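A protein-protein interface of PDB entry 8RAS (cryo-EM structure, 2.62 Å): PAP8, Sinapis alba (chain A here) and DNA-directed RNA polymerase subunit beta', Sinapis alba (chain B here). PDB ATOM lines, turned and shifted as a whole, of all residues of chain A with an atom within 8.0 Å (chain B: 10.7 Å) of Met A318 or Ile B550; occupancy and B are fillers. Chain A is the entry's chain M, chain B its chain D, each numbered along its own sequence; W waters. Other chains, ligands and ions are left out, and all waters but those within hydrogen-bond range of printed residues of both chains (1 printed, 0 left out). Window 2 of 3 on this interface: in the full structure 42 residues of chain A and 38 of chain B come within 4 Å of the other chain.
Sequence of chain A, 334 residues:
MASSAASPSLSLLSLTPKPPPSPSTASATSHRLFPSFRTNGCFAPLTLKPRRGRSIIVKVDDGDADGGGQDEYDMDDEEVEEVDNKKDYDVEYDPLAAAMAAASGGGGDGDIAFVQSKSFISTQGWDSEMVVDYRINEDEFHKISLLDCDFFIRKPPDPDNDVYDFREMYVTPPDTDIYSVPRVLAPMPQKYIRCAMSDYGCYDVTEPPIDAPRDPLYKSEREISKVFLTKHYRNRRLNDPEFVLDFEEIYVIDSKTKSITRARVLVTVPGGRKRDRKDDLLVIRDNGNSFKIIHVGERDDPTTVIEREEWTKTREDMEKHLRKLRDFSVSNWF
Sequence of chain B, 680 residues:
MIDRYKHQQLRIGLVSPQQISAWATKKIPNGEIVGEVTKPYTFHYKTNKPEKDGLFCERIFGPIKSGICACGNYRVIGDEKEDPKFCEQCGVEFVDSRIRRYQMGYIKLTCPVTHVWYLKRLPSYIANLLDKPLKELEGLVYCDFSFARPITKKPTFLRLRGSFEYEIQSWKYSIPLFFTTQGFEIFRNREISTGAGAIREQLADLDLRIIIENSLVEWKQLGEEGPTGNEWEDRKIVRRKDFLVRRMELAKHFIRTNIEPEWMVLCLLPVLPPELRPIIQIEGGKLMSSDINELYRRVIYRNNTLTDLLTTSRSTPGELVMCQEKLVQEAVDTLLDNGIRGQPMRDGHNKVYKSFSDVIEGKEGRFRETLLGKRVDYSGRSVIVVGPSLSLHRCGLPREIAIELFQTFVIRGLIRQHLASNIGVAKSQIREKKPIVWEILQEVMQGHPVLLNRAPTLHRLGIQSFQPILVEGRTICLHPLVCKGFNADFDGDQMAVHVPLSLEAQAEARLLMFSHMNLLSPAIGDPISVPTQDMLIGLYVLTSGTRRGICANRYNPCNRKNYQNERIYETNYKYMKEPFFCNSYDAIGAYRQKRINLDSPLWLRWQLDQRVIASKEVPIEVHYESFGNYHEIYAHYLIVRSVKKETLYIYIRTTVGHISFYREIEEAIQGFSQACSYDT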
ATOM      1  N   GLU A 307      16.564  29.298  20.229  1.00  0.00           N
ATOM      2  CA  GLU A 307      15.980  28.730  21.436  1.00  0.00           C
ATOM      3  C   GLU A 307      15.672  29.808  22.466  1.00  0.00           C
ATOM      4  O   GLU A 307      14.667  29.716  23.175  1.00  0.00           O
ATOM      5  CB  GLU A 307      16.916  27.675  22.020  1.00  0.00           C
ATOM      6  CG  GLU A 307      16.881  26.353  21.277  1.00  0.00           C
ATOM      7  CD  GLU A 307      17.587  25.244  22.026  1.00  0.00           C
ATOM      8  OE1 GLU A 307      18.575  25.534  22.732  1.00  0.00           O
ATOM      9  OE2 GLU A 307      17.154  24.079  21.907  1.00  0.00           O
ATOM     10  N   GLU A 309      14.823  32.980  21.815  1.00  0.00           N
ATOM     11  CA  GLU A 309      13.608  33.658  21.369  1.00  0.00           C
ATOM     12  C   GLU A 309      12.376  32.797  21.620  1.00  0.00           C
ATOM     13  O   GLU A 309      11.350  33.283  22.123  1.00  0.00           O
ATOM     14  CB  GLU A 309      13.720  34.015  19.889  1.00  0.00           C
ATOM     15  CG  GLU A 309      14.737  35.089  19.595  1.00  0.00           C
ATOM     16  CD  GLU A 309      14.360  36.432  20.184  1.00  0.00           C
ATOM     17  OE1 GLU A 309      13.153  36.750  20.223  1.00  0.00           O
ATOM     18  OE2 GLU A 309      15.274  37.171  20.605  1.00  0.00           O
ATOM     19  N   GLU A 310      12.465  31.508  21.281  1.00  0.00           N
ATOM     20  CA  GLU A 310      11.333  30.611  21.473  1.00  0.00           C
ATOM     21  C   GLU A 310      10.970  30.489  22.945  1.00  0.00           C
ATOM     22  O   GLU A 310       9.789  30.526  23.303  1.00  0.00           O
ATOM     23  CB  GLU A 310      11.649  29.236  20.887  1.00  0.00           C
ATOM     24  CG  GLU A 310      11.646  29.188  19.375  1.00  0.00           C
ATOM     25  CD  GLU A 310      12.082  27.842  18.838  1.00  0.00           C
ATOM     26  OE1 GLU A 310      12.762  27.100  19.577  1.00  0.00           O
ATOM     27  OE2 GLU A 310      11.746  27.525  17.678  1.00  0.00           O
ATOM     28  N   TRP A 311      11.974  30.348  23.813  1.00  0.00           N
ATOM     29  CA  TRP A 311      11.712  30.211  25.239  1.00  0.00           C
ATOM     30  C   TRP A 311      11.040  31.454  25.793  1.00  0.00           C
ATOM     31  O   TRP A 311      10.066  31.354  26.544  1.00  0.00           O
ATOM     32  CB  TRP A 311      13.014  29.927  25.987  1.00  0.00           C
ATOM     33  CG  TRP A 311      12.818  29.137  27.244  1.00  0.00           C
ATOM     34  CD1 TRP A 311      12.872  27.782  27.376  1.00  0.00           C
ATOM     35  CD2 TRP A 311      12.532  29.655  28.546  1.00  0.00           C
ATOM     36  NE1 TRP A 311      12.639  27.423  28.680  1.00  0.00           N
ATOM     37  CE2 TRP A 311      12.426  28.556  29.419  1.00  0.00           C
ATOM     38  CE3 TRP A 311      12.354  30.943  29.059  1.00  0.00           C
ATOM     39  CZ2 TRP A 311      12.152  28.705  30.775  1.00  0.00           C
ATOM     40  CZ3 TRP A 311      12.083  31.088  30.404  1.00  0.00           C
ATOM     41  CH2 TRP A 311      11.985  29.975  31.246  1.00  0.00           C
ATOM     42  N   THR A 312      11.532  32.636  25.420  1.00  0.00           N
ATOM     43  CA  THR A 312      10.927  33.868  25.914  1.00  0.00           C
ATOM     44  C   THR A 312       9.469  33.980  25.475  1.00  0.00           C
ATOM     45  O   THR A 312       8.567  34.190  26.305  1.00  0.00           O
ATOM     46  CB  THR A 312      11.744  35.067  25.430  1.00  0.00           C
ATOM     47  OG1 THR A 312      13.011  35.079  26.099  1.00  0.00           O
ATOM     48  CG2 THR A 312      11.023  36.364  25.719  1.00  0.00           C
ATOM     49  N   LYS A 313       9.215  33.814  24.173  1.00  0.00           N
ATOM     50  CA  LYS A 313       7.853  33.982  23.673  1.00  0.00           C
ATOM     51  C   LYS A 313       6.910  32.942  24.268  1.00  0.00           C
ATOM     52  O   LYS A 313       5.790  33.272  24.677  1.00  0.00           O
ATOM     53  CB  LYS A 313       7.835  33.915  22.148  1.00  0.00           C
ATOM     54  CG  LYS A 313       6.458  34.161  21.550  1.00  0.00           C
ATOM     55  CD  LYS A 313       6.508  34.258  20.038  1.00  0.00           C
ATOM     56  CE  LYS A 313       6.629  32.886  19.405  1.00  0.00           C
ATOM     57  NZ  LYS A 313       5.458  32.025  19.728  1.00  0.00           N
ATOM     58  N   THR A 314       7.348  31.683  24.338  1.00  0.00           N
ATOM     59  CA  THR A 314       6.492  30.630  24.870  1.00  0.00           C
ATOM     60  C   THR A 314       6.261  30.790  26.366  1.00  0.00           C
ATOM     61  O   THR A 314       5.181  30.456  26.857  1.00  0.00           O
ATOM     62  CB  THR A 314       7.099  29.262  24.573  1.00  0.00           C
ATOM     63  OG1 THR A 314       8.497  29.289  24.879  1.00  0.00           O
ATOM     64  CG2 THR A 314       6.916  28.910  23.110  1.00  0.00           C
ATOM     65  N   ARG A 315       7.252  31.295  27.105  1.00  0.00           N
ATOM     66  CA  ARG A 315       7.056  31.545  28.526  1.00  0.00           C
ATOM     67  C   ARG A 315       6.001  32.618  28.750  1.00  0.00           C
ATOM     68  O   ARG A 315       5.112  32.459  29.598  1.00  0.00           O
ATOM     69  CB  ARG A 315       8.386  31.944  29.167  1.00  0.00           C
ATOM     70  CG  ARG A 315       8.288  32.390  30.612  1.00  0.00           C
ATOM     71  CD  ARG A 315       8.270  31.202  31.556  1.00  0.00           C
ATOM     72  NE  ARG A 315       8.294  31.609  32.955  1.00  0.00           N
ATOM     73  CZ  ARG A 315       7.249  32.086  33.616  1.00  0.00           C
ATOM     74  NH1 ARG A 315       6.070  32.232  33.036  1.00  0.00           N
ATOM     75  NH2 ARG A 315       7.390  32.425  34.894  1.00  0.00           N
ATOM     76  N   GLU A 316       6.068  33.715  27.987  1.00  0.00           N
ATOM     77  CA  GLU A 316       5.027  34.733  28.120  1.00  0.00           C
ATOM     78  C   GLU A 316       3.661  34.192  27.710  1.00  0.00           C
ATOM     79  O   GLU A 316       2.650  34.483  28.363  1.00  0.00           O
ATOM     80  CB  GLU A 316       5.370  35.982  27.312  1.00  0.00           C
ATOM     81  CG  GLU A 316       6.330  36.921  28.012  1.00  0.00           C
ATOM     82  CD  GLU A 316       7.760  36.714  27.584  1.00  0.00           C
ATOM     83  OE1 GLU A 316       8.046  36.932  26.390  1.00  0.00           O
ATOM     84  OE2 GLU A 316       8.593  36.327  28.432  1.00  0.00           O
ATOM     85  N   ASP A 317       3.607  33.405  26.632  1.00  0.00           N
ATOM     86  CA  ASP A 317       2.333  32.840  26.200  1.00  0.00           C
ATOM     87  C   ASP A 317       1.742  31.923  27.264  1.00  0.00           C
ATOM     88  O   ASP A 317       0.536  31.970  27.536  1.00  0.00           O
ATOM     89  CB  ASP A 317       2.513  32.083  24.885  1.00  0.00           C
ATOM     90  CG  ASP A 317       2.475  32.995  23.680  1.00  0.00           C
ATOM     91  OD1 ASP A 317       2.504  34.230  23.864  1.00  0.00           O
ATOM     92  OD2 ASP A 317       2.415  32.477  22.545  1.00  0.00           O
ATOM     93  N   MET A 318       2.576  31.081  27.875  1.00  0.00           N
ATOM     94  CA  MET A 318       2.096  30.176  28.911  1.00  0.00           C
ATOM     95  C   MET A 318       1.617  30.942  30.135  1.00  0.00           C
ATOM     96  O   MET A 318       0.599  30.580  30.736  1.00  0.00           O
ATOM     97  CB  MET A 318       3.193  29.184  29.293  1.00  0.00           C
ATOM     98  CG  MET A 318       2.728  28.077  30.219  1.00  0.00           C
ATOM     99  SD  MET A 318       1.180  27.329  29.683  1.00  0.00           S
ATOM    100  CE  MET A 318       1.790  25.931  28.756  1.00  0.00           C
ATOM    101  N   GLU A 319       2.335  31.998  30.525  1.00  0.00           N
ATOM    102  CA  GLU A 319       1.873  32.803  31.652  1.00  0.00           C
ATOM    103  C   GLU A 319       0.537  33.466  31.342  1.00  0.00           C
ATOM    104  O   GLU A 319      -0.333  33.562  32.215  1.00  0.00           O
ATOM    105  CB  GLU A 319       2.918  33.850  32.028  1.00  0.00           C
ATOM    106  CG  GLU A 319       2.655  34.506  33.372  1.00  0.00           C
ATOM    107  CD  GLU A 319       3.920  34.739  34.167  1.00  0.00           C
ATOM    108  OE1 GLU A 319       5.006  34.797  33.555  1.00  0.00           O
ATOM    109  OE2 GLU A 319       3.830  34.862  35.406  1.00  0.00           O
ATOM    110  N   LYS A 320       0.356  33.936  30.105  1.00  0.00           N
ATOM    111  CA  LYS A 320      -0.923  34.531  29.728  1.00  0.00           C
ATOM    112  C   LYS A 320      -2.047  33.502  29.754  1.00  0.00           C
ATOM    113  O   LYS A 320      -3.170  33.814  30.169  1.00  0.00           O
ATOM    114  CB  LYS A 320      -0.818  35.176  28.348  1.00  0.00           C
ATOM    115  CG  LYS A 320      -0.246  36.581  28.368  1.00  0.00           C
ATOM    116  CD  LYS A 320       0.061  37.078  26.967  1.00  0.00           C
ATOM    117  CE  LYS A 320       0.750  38.431  27.005  1.00  0.00           C
ATOM    118  NZ  LYS A 320       1.159  38.884  25.648  1.00  0.00           N
ATOM    119  N   HIS A 321      -1.772  32.277  29.303  1.00  0.00           N
ATOM    120  CA  HIS A 321      -2.812  31.250  29.277  1.00  0.00           C
ATOM    121  C   HIS A 321      -3.213  30.821  30.684  1.00  0.00           C
ATOM    122  O   HIS A 321      -4.402  30.624  30.962  1.00  0.00           O
ATOM    123  CB  HIS A 321      -2.337  30.046  28.467  1.00  0.00           C
ATOM    124  CG  HIS A 321      -3.296  28.896  28.477  1.00  0.00           C
ATOM    125  ND1 HIS A 321      -3.042  27.722  29.151  1.00  0.00           N
ATOM    126  CD2 HIS A 321      -4.507  28.740  27.894  1.00  0.00           C
ATOM    127  CE1 HIS A 321      -4.055  26.892  28.983  1.00  0.00           C
ATOM    128  NE2 HIS A 321      -4.958  27.486  28.225  1.00  0.00           N
ATOM    129  N   LEU A 322      -2.240  30.663  31.582  1.00  0.00           N
ATOM    130  CA  LEU A 322      -2.526  30.181  32.928  1.00  0.00           C
ATOM    131  C   LEU A 322      -3.076  31.265  33.844  1.00  0.00           C
ATOM    132  O   LEU A 322      -3.653  30.939  34.886  1.00  0.00           O
ATOM    133  CB  LEU A 322      -1.264  29.585  33.553  1.00  0.00           C
ATOM    134  CG  LEU A 322      -0.696  28.320  32.909  1.00  0.00           C
ATOM    135  CD1 LEU A 322       0.564  27.881  33.630  1.00  0.00           C
ATOM    136  CD2 LEU A 322      -1.729  27.208  32.903  1.00  0.00           C
ATOM    137  N   ARG A 323      -2.912  32.540  33.481  1.00  0.00           N
ATOM    138  CA  ARG A 323      -3.333  33.628  34.357  1.00  0.00           C
ATOM    139  C   ARG A 323      -4.841  33.619  34.584  1.00  0.00           C
ATOM    140  O   ARG A 323      -5.314  34.083  35.628  1.00  0.00           O
ATOM    141  CB  ARG A 323      -2.873  34.962  33.764  1.00  0.00           C
ATOM    142  CG  ARG A 323      -3.453  36.205  34.414  1.00  0.00           C
ATOM    143  CD  ARG A 323      -2.788  36.496  35.746  1.00  0.00           C
ATOM    144  NE  ARG A 323      -3.749  36.936  36.750  1.00  0.00           N
ATOM    145  CZ  ARG A 323      -3.439  37.222  38.007  1.00  0.00           C
ATOM    146  NH1 ARG A 323      -2.197  37.124  38.453  1.00  0.00           N
ATOM    147  NH2 ARG A 323      -4.399  37.617  38.838  1.00  0.00           N
ATOM    148  N   LYS A 324      -5.607  33.075  33.641  1.00  0.00           N
ATOM    149  CA  LYS A 324      -7.060  33.077  33.751  1.00  0.00           C
ATOM    150  C   LYS A 324      -7.592  32.041  34.735  1.00  0.00           C
ATOM    151  O   LYS A 324      -8.787  32.071  35.045  1.00  0.00           O
ATOM    152  CB  LYS A 324      -7.688  32.860  32.371  1.00  0.00           C
ATOM    153  CG  LYS A 324      -8.031  31.419  32.041  1.00  0.00           C
ATOM    154  CD  LYS A 324      -8.768  31.332  30.714  1.00  0.00           C
ATOM    155  CE  LYS A 324      -7.831  31.609  29.548  1.00  0.00           C
ATOM    156  NZ  LYS A 324      -8.518  31.475  28.235  1.00  0.00           N
ATOM    157  N   PHE A 328      -4.159  30.706  40.154  1.00  0.00           N
ATOM    158  CA  PHE A 328      -2.885  31.133  39.584  1.00  0.00           C
ATOM    159  C   PHE A 328      -2.043  31.900  40.596  1.00  0.00           C
ATOM    160  O   PHE A 328      -0.811  31.812  40.569  1.00  0.00           O
ATOM    161  CB  PHE A 328      -3.148  31.982  38.339  1.00  0.00           C
ATOM    162  CG  PHE A 328      -1.911  32.556  37.713  1.00  0.00           C
ATOM    163  CD1 PHE A 328      -1.184  31.824  36.790  1.00  0.00           C
ATOM    164  CD2 PHE A 328      -1.490  33.839  38.023  1.00  0.00           C
ATOM    165  CE1 PHE A 328      -0.052  32.351  36.204  1.00  0.00           C
ATOM    166  CE2 PHE A 328      -0.357  34.371  37.442  1.00  0.00           C
ATOM    167  CZ  PHE A 328       0.361  33.627  36.530  1.00  0.00           C
ATOM    168  N   TRP A 333       5.669  28.263  39.203  1.00  0.00           N
ATOM    169  CA  TRP A 333       6.259  27.831  37.947  1.00  0.00           C
ATOM    170  C   TRP A 333       7.292  26.747  38.229  1.00  0.00           C
ATOM    171  O   TRP A 333       7.932  26.740  39.282  1.00  0.00           O
ATOM    172  CB  TRP A 333       6.910  29.005  37.212  1.00  0.00           C
ATOM    173  CG  TRP A 333       7.876  28.585  36.142  1.00  0.00           C
ATOM    174  CD1 TRP A 333       9.215  28.371  36.285  1.00  0.00           C
ATOM    175  CD2 TRP A 333       7.574  28.319  34.767  1.00  0.00           C
ATOM    176  NE1 TRP A 333       9.765  27.989  35.088  1.00  0.00           N
ATOM    177  CE2 TRP A 333       8.777  27.950  34.139  1.00  0.00           C
ATOM    178  CE3 TRP A 333       6.402  28.360  34.006  1.00  0.00           C
ATOM    179  CZ2 TRP A 333       8.845  27.624  32.789  1.00  0.00           C
ATOM    180  CZ3 TRP A 333       6.472  28.034  32.667  1.00  0.00           C
ATOM    181  CH2 TRP A 333       7.684  27.671  32.072  1.00  0.00           C
ATOM    182  N   PHE A 334       7.436  25.818  37.291  1.00  0.00           N
ATOM    183  CA  PHE A 334       8.470  24.794  37.398  1.00  0.00           C
ATOM    184  C   PHE A 334       8.783  24.191  36.034  1.00  0.00           C
ATOM    185  O   PHE A 334       8.059  24.420  35.067  1.00  0.00           O
ATOM    186  CB  PHE A 334       8.052  23.693  38.381  1.00  0.00           C
ATOM    187  CG  PHE A 334       6.697  23.113  38.104  1.00  0.00           C
ATOM    188  CD1 PHE A 334       6.546  22.072  37.206  1.00  0.00           C
ATOM    189  CD2 PHE A 334       5.575  23.607  38.743  1.00  0.00           C
ATOM    190  CE1 PHE A 334       5.307  21.540  36.949  1.00  0.00           C
ATOM    191  CE2 PHE A 334       4.332  23.077  38.489  1.00  0.00           C
ATOM    192  CZ  PHE A 334       4.198  22.043  37.592  1.00  0.00           C
ATOM    193  N   THR B 546       9.373  20.759  15.560  1.00  0.00           N
ATOM    194  CA  THR B 546      10.035  20.551  16.837  1.00  0.00           C
ATOM    195  C   THR B 546       9.200  21.095  17.989  1.00  0.00           C
ATOM    196  O   THR B 546       8.379  22.001  17.821  1.00  0.00           O
ATOM    197  CB  THR B 546      11.398  21.239  16.848  1.00  0.00           C
ATOM    198  OG1 THR B 546      11.281  22.535  16.247  1.00  0.00           O
ATOM    199  CG2 THR B 546      12.401  20.432  16.070  1.00  0.00           C
ATOM    200  N   ARG B 547       9.417  20.524  19.169  1.00  0.00           N
ATOM    201  CA  ARG B 547       8.985  21.177  20.394  1.00  0.00           C
ATOM    202  C   ARG B 547       9.860  22.399  20.633  1.00  0.00           C
ATOM    203  O   ARG B 547      11.084  22.339  20.491  1.00  0.00           O
ATOM    204  CB  ARG B 547       9.071  20.214  21.575  1.00  0.00           C
ATOM    205  CG  ARG B 547       7.821  19.381  21.777  1.00  0.00           C
ATOM    206  CD  ARG B 547       8.099  18.142  22.606  1.00  0.00           C
ATOM    207  NE  ARG B 547       6.872  17.579  23.156  1.00  0.00           N
ATOM    208  CZ  ARG B 547       6.707  16.302  23.470  1.00  0.00           C
ATOM    209  NH1 ARG B 547       7.675  15.417  23.301  1.00  0.00           N
ATOM    210  NH2 ARG B 547       5.540  15.902  23.967  1.00  0.00           N
ATOM    211  N   ARG B 548       9.232  23.516  20.979  1.00  0.00           N
ATOM    212  CA  ARG B 548       9.926  24.792  21.017  1.00  0.00           C
ATOM    213  C   ARG B 548       9.690  25.495  22.344  1.00  0.00           C
ATOM    214  O   ARG B 548       8.642  25.336  22.976  1.00  0.00           O
ATOM    215  CB  ARG B 548       9.476  25.697  19.865  1.00  0.00           C
ATOM    216  CG  ARG B 548       8.005  25.575  19.523  1.00  0.00           C
ATOM    217  CD  ARG B 548       7.632  26.505  18.386  1.00  0.00           C
ATOM    218  NE  ARG B 548       8.226  27.825  18.553  1.00  0.00           N
ATOM    219  CZ  ARG B 548       7.562  28.902  18.947  1.00  0.00           C
ATOM    220  NH1 ARG B 548       6.273  28.852  19.237  1.00  0.00           N
ATOM    221  NH2 ARG B 548       8.210  30.059  19.057  1.00  0.00           N
ATOM    222  N   GLY B 549      10.684  26.271  22.756  1.00  0.00           N
ATOM    223  CA  GLY B 549      10.520  27.123  23.921  1.00  0.00           C
ATOM    224  C   GLY B 549      10.510  26.332  25.211  1.00  0.00           C
ATOM    225  O   GLY B 549      11.355  25.462  25.442  1.00  0.00           O
ATOM    226  N   ILE B 550       9.541  26.645  26.075  1.00  0.00           N
ATOM    227  CA  ILE B 550       9.433  25.982  27.369  1.00  0.00           C
ATOM    228  C   ILE B 550       9.039  24.521  27.253  1.00  0.00           C
ATOM    229  O   ILE B 550       9.162  23.778  28.231  1.00  0.00           O
ATOM    230  CB  ILE B 550       8.429  26.728  28.270  1.00  0.00           C
ATOM    231  CG1 ILE B 550       7.046  26.756  27.622  1.00  0.00           C
ATOM    232  CG2 ILE B 550       8.913  28.138  28.549  1.00  0.00           C
ATOM    233  CD1 ILE B 550       5.916  26.812  28.613  1.00  0.00           C
ATOM    234  N   CYS B 551       8.571  24.088  26.086  1.00  0.00           N
ATOM    235  CA  CYS B 551       8.266  22.685  25.842  1.00  0.00           C
ATOM    236  C   CYS B 551       9.469  21.906  25.328  1.00  0.00           C
ATOM    237  O   CYS B 551       9.347  20.704  25.076  1.00  0.00           O
ATOM    238  CB  CYS B 551       7.108  22.560  24.849  1.00  0.00           C
ATOM    239  SG  CYS B 551       5.499  23.044  25.514  1.00  0.00           S
ATOM    240  N   ALA B 552      10.616  22.555  25.168  1.00  0.00           N
ATOM    241  CA  ALA B 552      11.839  21.909  24.713  1.00  0.00           C
ATOM    242  C   ALA B 552      12.951  21.939  25.746  1.00  0.00           C
ATOM    243  O   ALA B 552      13.725  20.984  25.835  1.00  0.00           O
ATOM    244  CB  ALA B 552      12.335  22.565  23.420  1.00  0.00           C
ATOM    245  N   ASN B 553      13.056  23.012  26.523  1.00  0.00           N
ATOM    246  CA  ASN B 553      14.080  23.142  27.547  1.00  0.00           C
ATOM    247  C   ASN B 553      13.424  23.433  28.886  1.00  0.00           C
ATOM    248  O   ASN B 553      12.482  24.227  28.965  1.00  0.00           O
ATOM    249  CB  ASN B 553      15.079  24.258  27.212  1.00  0.00           C
ATOM    250  CG  ASN B 553      15.687  24.105  25.836  1.00  0.00           C
ATOM    251  OD1 ASN B 553      16.429  23.162  25.575  1.00  0.00           O
ATOM    252  ND2 ASN B 553      15.378  25.041  24.947  1.00  0.00           N
ATOM    253  N   ARG B 554      13.925  22.784  29.937  1.00  0.00           N
ATOM    254  CA  ARG B 554      13.437  23.070  31.280  1.00  0.00           C
ATOM    255  C   ARG B 554      13.845  24.460  31.740  1.00  0.00           C
ATOM    256  O   ARG B 554      13.083  25.127  32.447  1.00  0.00           O
ATOM    257  CB  ARG B 554      13.950  22.018  32.262  1.00  0.00           C
ATOM    258  CG  ARG B 554      13.057  21.812  33.470  1.00  0.00           C
ATOM    259  CD  ARG B 554      13.867  21.365  34.670  1.00  0.00           C
ATOM    260  NE  ARG B 554      13.345  21.889  35.924  1.00  0.00           N
ATOM    261  CZ  ARG B 554      13.458  21.274  37.094  1.00  0.00           C
ATOM    262  NH1 ARG B 554      14.060  20.102  37.202  1.00  0.00           N
ATOM    263  NH2 ARG B 554      12.955  21.850  38.181  1.00  0.00           N
ATOM    264  N   TYR B 555      15.031  24.912  31.351  1.00  0.00           N
ATOM    265  CA  TYR B 555      15.564  26.193  31.778  1.00  0.00           C
ATOM    266  C   TYR B 555      15.759  27.102  30.573  1.00  0.00           C
ATOM    267  O   TYR B 555      15.870  26.646  29.432  1.00  0.00           O
ATOM    268  CB  TYR B 555      16.894  26.018  32.520  1.00  0.00           C
ATOM    269  CG  TYR B 555      16.789  25.163  33.759  1.00  0.00           C
ATOM    270  CD1 TYR B 555      16.083  25.600  34.871  1.00  0.00           C
ATOM    271  CD2 TYR B 555      17.386  23.911  33.812  1.00  0.00           C
ATOM    272  CE1 TYR B 555      15.983  24.819  36.003  1.00  0.00           C
ATOM    273  CE2 TYR B 555      17.289  23.123  34.940  1.00  0.00           C
ATOM    274  CZ  TYR B 555      16.587  23.581  36.032  1.00  0.00           C
ATOM    275  OH  TYR B 555      16.491  22.798  37.158  1.00  0.00           O
ATOM    276  N   ASN B 556      15.786  28.399  30.845  1.00  0.00           N
ATOM    277  CA  ASN B 556      16.072  29.377  29.809  1.00  0.00           C
ATOM    278  C   ASN B 556      17.483  29.152  29.274  1.00  0.00           C
ATOM    279  O   ASN B 556      18.441  29.138  30.058  1.00  0.00           O
ATOM    280  CB  ASN B 556      15.939  30.788  30.379  1.00  0.00           C
ATOM    281  CG  ASN B 556      15.812  31.851  29.311  1.00  0.00           C
ATOM    282  OD1 ASN B 556      15.856  31.563  28.117  1.00  0.00           O
ATOM    283  ND2 ASN B 556      15.654  33.096  29.739  1.00  0.00           N
ATOM    284  N   PRO B 557      17.658  28.970  27.963  1.00  0.00           N
ATOM    285  CA  PRO B 557      19.013  28.787  27.426  1.00  0.00           C
ATOM    286  C   PRO B 557      19.827  30.069  27.482  1.00  0.00           C
ATOM    287  O   PRO B 557      20.200  30.621  26.443  1.00  0.00           O
ATOM    288  CB  PRO B 557      18.767  28.339  25.978  1.00  0.00           C
ATOM    289  CG  PRO B 557      17.315  27.980  25.905  1.00  0.00           C
ATOM    290  CD  PRO B 557      16.627  28.815  26.924  1.00  0.00           C
HETATM  291  O   HOH W   1      13.919  26.714  23.929  1.00  0.00           O
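The side-chain carboxylate (OE1) of Glu A319 lies within salt-bridge range of the guanidinium group (NH1) of Arg A315 (2.8 Å).
The side-chain hydroxyl of Tyr B555 sits close to the guanidinium group of Arg B554.
Water W1 lies within hydrogen-bond range of ND2 of Asn B553 (2.4 Å), O of Glu A307 (3.2 Å) and O of Gly B549 (3.2 Å).
The indole nitrogen of Trp A311 lies within hydrogen-bond range of the backbone carbonyl oxygen of Asn B553, 3.2 Å away.
N of Ile B550 lies within hydrogen-bond range of OG1 of Thr A314 (3.1 Å).
NE1 of Trp A311 sits at hydrogen-bond distance from O of Tyr B555, at 3.4 Å.
NE of Arg B548 lies within salt-bridge range of OE2 of Glu A310, 3.6 Å away.
The side-chain amino group (NZ) of Lys A313 lies close to the guanidinium group (NH1) of Arg B548 (3.3 Å).
Of the 20 printed residues of chain A, 8 touch a printed residue of chain B.
Printed residues of chain B that touch a printed residue of chain A: Arg B548, Gly B549, Ile B550, Asn B553, Tyr B555, Asn B556 and Pro B557.
Hydrophobic or aromatic side chains of chain B that line the printed part of chain A: Ile B550 and Pro B557.
Among the printed residues, 17 pairs touch across the chains.
Among the printed residues, Asp or Glu carboxylates within 4 Å of a Lys or Arg side-chain nitrogen of the other chain: Glu A310 with Arg B548.
Among the printed residues, merely in contact across the chains: Thr A314 with Gly B549, Trp A311 with Gly B549, Glu A310 with Gly B549, Trp A311 with Asn B556, Trp A311 with Ile B550, Glu A307 with Asn B553, Met A318 with Ile B550, Trp A333 with Ile B550, Trp A311 with Pro B557, Arg A315 with Ile B550, Glu A307 with Pro B557 and Thr A314 with Arg B548.
Printed residues of chain B within 4 Å of Glu A307: Asn B553 (3.6 Å) and Pro B557 (3.9 Å).
Trp A311 touches just these residues of chain B: Gly B549 (3.4 Å), Ile B550 (3.6 Å), Asn B553 (3.2 Å), Tyr B555 (3.4 Å), Asn B556 (3.6 Å) and Pro B557 (3.8 Å).
Of the printed residues of chain B, Lys A313 touches Arg B548.
Of chain B, only Ile B550 comes within 4 Å of Met A318.
Printed residues of chain B within 4 Å of Trp A333: Ile B550 (3.8 Å).
Of chain A, only Glu A310, Trp A311 and Thr A314 come within 4 Å of Gly B549.
Of the printed residues of chain A, Asn B553 touches Glu A307 and Trp A311.
The nearest residue of chain B that does not touch Met A318 is Cys B551 (5.7 Å).
The nearest printed residue of chain A that does not touch Pro B557 is Thr A312 (6.5 Å).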
